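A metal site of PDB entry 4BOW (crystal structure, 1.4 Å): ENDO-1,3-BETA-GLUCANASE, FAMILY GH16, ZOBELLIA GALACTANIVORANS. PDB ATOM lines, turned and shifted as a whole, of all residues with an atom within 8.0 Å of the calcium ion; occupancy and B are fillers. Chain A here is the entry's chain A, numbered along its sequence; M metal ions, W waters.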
ATOM      1  N   ASP A  17      16.785 -28.813 -30.061  1.00  0.00           N
ATOM      2  CA  ASP A  17      16.354 -29.645 -28.914  1.00  0.00           C
ATOM      3  C   ASP A  17      14.876 -29.495 -28.810  1.00  0.00           C
ATOM      4  O   ASP A  17      14.381 -28.370 -28.619  1.00  0.00           O
ATOM      5  CB  ASP A  17      17.080 -29.220 -27.590  1.00  0.00           C
ATOM      6  CG  ASP A  17      17.012 -30.288 -26.505  1.00  0.00           C
ATOM      7  OD1 ASP A  17      16.087 -31.194 -26.692  1.00  0.00           O
ATOM      8  OD2 ASP A  17      17.804 -30.284 -25.518  1.00  0.00           O
ATOM      9  N   GLU A  18      14.181 -30.643 -28.985  1.00  0.00           N
ATOM     10  CA  GLU A  18      12.745 -30.624 -28.815  1.00  0.00           C
ATOM     11  C   GLU A  18      12.299 -30.913 -27.381  1.00  0.00           C
ATOM     12  O   GLU A  18      11.077 -30.862 -27.094  1.00  0.00           O
ATOM     13  CB  GLU A  18      12.117 -31.676 -29.740  1.00  0.00           C
ATOM     14  CG  GLU A  18      12.574 -31.490 -31.191  1.00  0.00           C
ATOM     15  CD  GLU A  18      11.888 -30.287 -31.821  1.00  0.00           C
ATOM     16  OE1 GLU A  18      10.759 -29.869 -31.509  1.00  0.00           O
ATOM     17  OE2 GLU A  18      12.502 -29.713 -32.721  1.00  0.00           O
ATOM     18  N   PHE A  19      13.233 -31.243 -26.495  1.00  0.00           N
ATOM     19  CA  PHE A  19      12.944 -31.398 -25.049  1.00  0.00           C
ATOM     20  C   PHE A  19      11.943 -32.540 -24.797  1.00  0.00           C
ATOM     21  O   PHE A  19      11.093 -32.381 -23.883  1.00  0.00           O
ATOM     22  CB  PHE A  19      12.493 -30.027 -24.438  1.00  0.00           C
ATOM     23  CG  PHE A  19      13.618 -29.014 -24.496  1.00  0.00           C
ATOM     24  CD1 PHE A  19      14.810 -29.211 -23.815  1.00  0.00           C
ATOM     25  CD2 PHE A  19      13.462 -27.843 -25.249  1.00  0.00           C
ATOM     26  CE1 PHE A  19      15.885 -28.323 -23.877  1.00  0.00           C
ATOM     27  CE2 PHE A  19      14.535 -26.925 -25.289  1.00  0.00           C
ATOM     28  CZ  PHE A  19      15.743 -27.150 -24.626  1.00  0.00           C
ATOM     29  N   GLU A  20      12.050 -33.587 -25.573  1.00  0.00           N
ATOM     30  CA  GLU A  20      11.102 -34.726 -25.426  1.00  0.00           C
ATOM     31  C   GLU A  20      11.911 -35.811 -24.709  1.00  0.00           C
ATOM     32  O   GLU A  20      12.026 -36.979 -25.182  1.00  0.00           O
ATOM     33  CB  GLU A  20      10.631 -35.190 -26.816  1.00  0.00           C
ATOM     34  CG  GLU A  20       9.891 -34.120 -27.608  1.00  0.00           C
ATOM     35  CD  GLU A  20       8.543 -33.537 -27.079  1.00  0.00           C
ATOM     36  OE1 GLU A  20       7.804 -34.337 -26.436  1.00  0.00           O
ATOM     37  OE2 GLU A  20       8.245 -32.278 -27.262  1.00  0.00           O
ATOM     38  N   TYR A  21      12.439 -35.480 -23.580  1.00  0.00           N
ATOM     39  CA  TYR A  21      13.022 -36.427 -22.665  1.00  0.00           C
ATOM     40  C   TYR A  21      12.722 -35.877 -21.245  1.00  0.00           C
ATOM     41  O   TYR A  21      11.977 -34.863 -21.065  1.00  0.00           O
ATOM     42  CB  TYR A  21      14.512 -36.593 -22.904  1.00  0.00           C
ATOM     43  CG  TYR A  21      15.300 -35.210 -22.970  1.00  0.00           C
ATOM     44  CD1 TYR A  21      15.429 -34.554 -24.201  1.00  0.00           C
ATOM     45  CD2 TYR A  21      15.891 -34.561 -21.816  1.00  0.00           C
ATOM     46  CE1 TYR A  21      16.063 -33.267 -24.280  1.00  0.00           C
ATOM     47  CE2 TYR A  21      16.605 -33.352 -21.904  1.00  0.00           C
ATOM     48  CZ  TYR A  21      16.660 -32.747 -23.162  1.00  0.00           C
ATOM     49  OH  TYR A  21      17.332 -31.532 -23.214  1.00  0.00           O
ATOM     50  N   VAL A  59      13.577 -30.747 -17.534  1.00  0.00           N
ATOM     51  CA  VAL A  59      12.866 -31.041 -18.768  1.00  0.00           C
ATOM     52  C   VAL A  59      11.795 -32.061 -18.434  1.00  0.00           C
ATOM     53  O   VAL A  59      12.156 -33.093 -17.788  1.00  0.00           O
ATOM     54  CB  VAL A  59      13.828 -31.579 -19.844  1.00  0.00           C
ATOM     55  CG1 VAL A  59      13.102 -31.752 -21.155  1.00  0.00           C
ATOM     56  CG2 VAL A  59      14.999 -30.502 -20.061  1.00  0.00           C
ATOM     57  N   SER A  60      10.579 -31.795 -18.817  1.00  0.00           N
ATOM     58  CA  SER A  60       9.473 -32.771 -18.562  1.00  0.00           C
ATOM     59  C   SER A  60       8.310 -32.460 -19.468  1.00  0.00           C
ATOM     60  O   SER A  60       8.113 -31.304 -19.919  1.00  0.00           O
ATOM     61  CB  SER A  60       9.025 -32.694 -17.083  1.00  0.00           C
ATOM     62  OG  SER A  60       8.581 -31.356 -16.758  1.00  0.00           O
ATOM     63  N   ASP A  61       7.507 -33.476 -19.765  1.00  0.00           N
ATOM     64  CA  ASP A  61       6.221 -33.175 -20.503  1.00  0.00           C
ATOM     65  C   ASP A  61       6.491 -32.359 -21.855  1.00  0.00           C
ATOM     66  O   ASP A  61       5.657 -31.537 -22.243  1.00  0.00           O
ATOM     67  CB  ASP A  61       5.275 -32.410 -19.558  1.00  0.00           C
ATOM     68  CG  ASP A  61       3.821 -32.433 -19.984  1.00  0.00           C
ATOM     69  OD1 ASP A  61       3.459 -33.338 -20.768  1.00  0.00           O
ATOM     70  OD2 ASP A  61       3.041 -31.526 -19.538  1.00  0.00           O
ATOM     71  N   GLY A  62       7.614 -32.640 -22.483  1.00  0.00           N
ATOM     72  CA  GLY A  62       7.998 -32.023 -23.780  1.00  0.00           C
ATOM     73  C   GLY A  62       8.543 -30.615 -23.764  1.00  0.00           C
ATOM     74  O   GLY A  62       8.760 -30.032 -24.833  1.00  0.00           O
ATOM     75  N   THR A  63       8.850 -30.103 -22.594  1.00  0.00           N
ATOM     76  CA  THR A  63       9.345 -28.727 -22.495  1.00  0.00           C
ATOM     77  C   THR A  63      10.435 -28.559 -21.455  1.00  0.00           C
ATOM     78  O   THR A  63      10.508 -29.304 -20.443  1.00  0.00           O
ATOM     79  CB  THR A  63       8.255 -27.718 -22.201  1.00  0.00           C
ATOM     80  OG1 THR A  63       7.764 -27.858 -20.859  1.00  0.00           O
ATOM     81  CG2 THR A  63       7.088 -27.793 -23.147  1.00  0.00           C
ATOM     82  N   LEU A  64      11.397 -27.673 -21.763  1.00  0.00           N
ATOM     83  CA  LEU A  64      12.391 -27.196 -20.813  1.00  0.00           C
ATOM     84  C   LEU A  64      11.718 -26.155 -19.935  1.00  0.00           C
ATOM     85  O   LEU A  64      11.037 -25.257 -20.419  1.00  0.00           O
ATOM     86  CB  LEU A  64      13.549 -26.564 -21.618  1.00  0.00           C
ATOM     87  CG  LEU A  64      14.523 -25.768 -20.717  1.00  0.00           C
ATOM     88  CD1 LEU A  64      15.348 -26.627 -19.757  1.00  0.00           C
ATOM     89  CD2 LEU A  64      15.518 -25.021 -21.624  1.00  0.00           C
ATOM     90  N   ARG A 101      10.374 -21.618 -29.348  1.00  0.00           N
ATOM     91  CA  ARG A 101       8.935 -21.504 -29.008  1.00  0.00           C
ATOM     92  C   ARG A 101       8.797 -21.535 -27.498  1.00  0.00           C
ATOM     93  O   ARG A 101       9.314 -22.483 -26.887  1.00  0.00           O
ATOM     94  CB  ARG A 101       8.193 -22.667 -29.697  1.00  0.00           C
ATOM     95  CG  ARG A 101       6.704 -22.582 -29.401  1.00  0.00           C
ATOM     96  CD  ARG A 101       5.956 -23.590 -30.268  1.00  0.00           C
ATOM     97  NE  ARG A 101       4.480 -23.390 -30.214  1.00  0.00           N
ATOM     98  CZ  ARG A 101       3.647 -24.189 -29.581  1.00  0.00           C
ATOM     99  NH1 ARG A 101       4.132 -25.269 -28.981  1.00  0.00           N
ATOM    100  NH2 ARG A 101       2.326 -23.930 -29.628  1.00  0.00           N
ATOM    101  N   PHE A 186       2.061 -20.022 -26.060  1.00  0.00           N
ATOM    102  CA  PHE A 186       3.381 -20.074 -26.728  1.00  0.00           C
ATOM    103  C   PHE A 186       3.439 -19.071 -27.898  1.00  0.00           C
ATOM    104  O   PHE A 186       2.473 -18.870 -28.644  1.00  0.00           O
ATOM    105  CB  PHE A 186       3.590 -21.452 -27.345  1.00  0.00           C
ATOM    106  CG  PHE A 186       3.952 -22.491 -26.348  1.00  0.00           C
ATOM    107  CD1 PHE A 186       5.233 -22.489 -25.727  1.00  0.00           C
ATOM    108  CD2 PHE A 186       3.024 -23.510 -25.995  1.00  0.00           C
ATOM    109  CE1 PHE A 186       5.621 -23.476 -24.840  1.00  0.00           C
ATOM    110  CE2 PHE A 186       3.427 -24.514 -25.078  1.00  0.00           C
ATOM    111  CZ  PHE A 186       4.693 -24.474 -24.475  1.00  0.00           C
ATOM    112  N   ILE A 249      10.178 -23.544 -22.425  1.00  0.00           N
ATOM    113  CA  ILE A 249      10.635 -23.577 -23.831  1.00  0.00           C
ATOM    114  C   ILE A 249      10.239 -24.943 -24.444  1.00  0.00           C
ATOM    115  O   ILE A 249      10.741 -25.973 -23.973  1.00  0.00           O
ATOM    116  CB  ILE A 249      12.132 -23.298 -23.838  1.00  0.00           C
ATOM    117  CG1 ILE A 249      12.379 -21.827 -23.371  1.00  0.00           C
ATOM    118  CG2 ILE A 249      12.690 -23.494 -25.261  1.00  0.00           C
ATOM    119  CD1 ILE A 249      13.726 -21.634 -22.985  1.00  0.00           C
ATOM    120  N   ASP A 250       9.413 -24.882 -25.498  1.00  0.00           N
ATOM    121  CA  ASP A 250       9.001 -26.121 -26.163  1.00  0.00           C
ATOM    122  C   ASP A 250      10.131 -26.654 -27.032  1.00  0.00           C
ATOM    123  O   ASP A 250      10.350 -27.896 -27.114  1.00  0.00           O
ATOM    124  CB  ASP A 250       7.776 -25.767 -27.005  1.00  0.00           C
ATOM    125  CG  ASP A 250       7.197 -26.973 -27.698  1.00  0.00           C
ATOM    126  OD1 ASP A 250       7.371 -28.135 -27.242  1.00  0.00           O
ATOM    127  OD2 ASP A 250       6.528 -26.691 -28.677  1.00  0.00           O
ATOM    128  N   TYR A 251      10.872 -25.788 -27.737  1.00  0.00           N
ATOM    129  CA  TYR A 251      11.982 -26.270 -28.559  1.00  0.00           C
ATOM    130  C   TYR A 251      12.916 -25.109 -28.892  1.00  0.00           C
ATOM    131  O   TYR A 251      12.493 -23.925 -28.845  1.00  0.00           O
ATOM    132  CB  TYR A 251      11.458 -26.899 -29.923  1.00  0.00           C
ATOM    133  CG  TYR A 251      10.599 -26.033 -30.796  1.00  0.00           C
ATOM    134  CD1 TYR A 251      11.123 -24.940 -31.498  1.00  0.00           C
ATOM    135  CD2 TYR A 251       9.264 -26.308 -30.910  1.00  0.00           C
ATOM    136  CE1 TYR A 251      10.331 -24.200 -32.394  1.00  0.00           C
ATOM    137  CE2 TYR A 251       8.484 -25.615 -31.849  1.00  0.00           C
ATOM    138  CZ  TYR A 251       8.987 -24.541 -32.496  1.00  0.00           C
ATOM    139  OH  TYR A 251       8.246 -23.769 -33.378  1.00  0.00           O
ATOM    140  N   VAL A 252      14.134 -25.491 -29.246  1.00  0.00           N
ATOM    141  CA  VAL A 252      15.060 -24.590 -29.915  1.00  0.00           C
ATOM    142  C   VAL A 252      15.425 -25.252 -31.226  1.00  0.00           C
ATOM    143  O   VAL A 252      15.763 -26.461 -31.201  1.00  0.00           O
ATOM    144  CB  VAL A 252      16.380 -24.439 -29.064  1.00  0.00           C
ATOM    145  CG1 VAL A 252      17.411 -23.682 -29.823  1.00  0.00           C
ATOM    146  CG2 VAL A 252      16.018 -23.788 -27.734  1.00  0.00           C
ATOM    147  N   ARG A 253      15.330 -24.543 -32.352  1.00  0.00           N
ATOM    148  CA  ARG A 253      15.795 -25.083 -33.608  1.00  0.00           C
ATOM    149  C   ARG A 253      16.656 -24.058 -34.337  1.00  0.00           C
ATOM    150  O   ARG A 253      16.293 -22.865 -34.321  1.00  0.00           O
ATOM    151  CB  ARG A 253      14.574 -25.344 -34.538  1.00  0.00           C
ATOM    152  CG  ARG A 253      13.643 -26.494 -33.994  1.00  0.00           C
ATOM    153  CD  ARG A 253      12.293 -26.477 -34.763  1.00  0.00           C
ATOM    154  NE  ARG A 253      11.445 -27.492 -34.133  1.00  0.00           N
ATOM    155  CZ  ARG A 253      10.128 -27.620 -34.349  1.00  0.00           C
ATOM    156  NH1 ARG A 253       9.540 -26.765 -35.153  1.00  0.00           N
ATOM    157  NH2 ARG A 253       9.420 -28.550 -33.674  1.00  0.00           N
HETATM  158 CA    CA M   1       8.978 -29.857 -27.079  1.00  0.00          CA
HETATM  159  O   HOH W   1       8.906 -29.932 -29.488  1.00  0.00           O
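The calcium ion is bound by O of Gly 62 (2.3 Å), O of Glu 18 (2.3 Å), OD1 of Asp 250 (2.4 Å), O of Asp 250 (2.4 Å), water W1 (2.4 Å) and OE2 of Glu 20 (2.5 Å). The calcium ion has six donor atoms within binding distance.
OE2 of Glu 18 lies within salt-bridge range of NE of Arg 253 (2.8 Å). OD2 of Asp 250 lies within salt-bridge range of NH1 of Arg 101, 2.8 Å away.
The nearest printed residue that does not touch the calcium ion is Phe 19 (4.4 Å).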
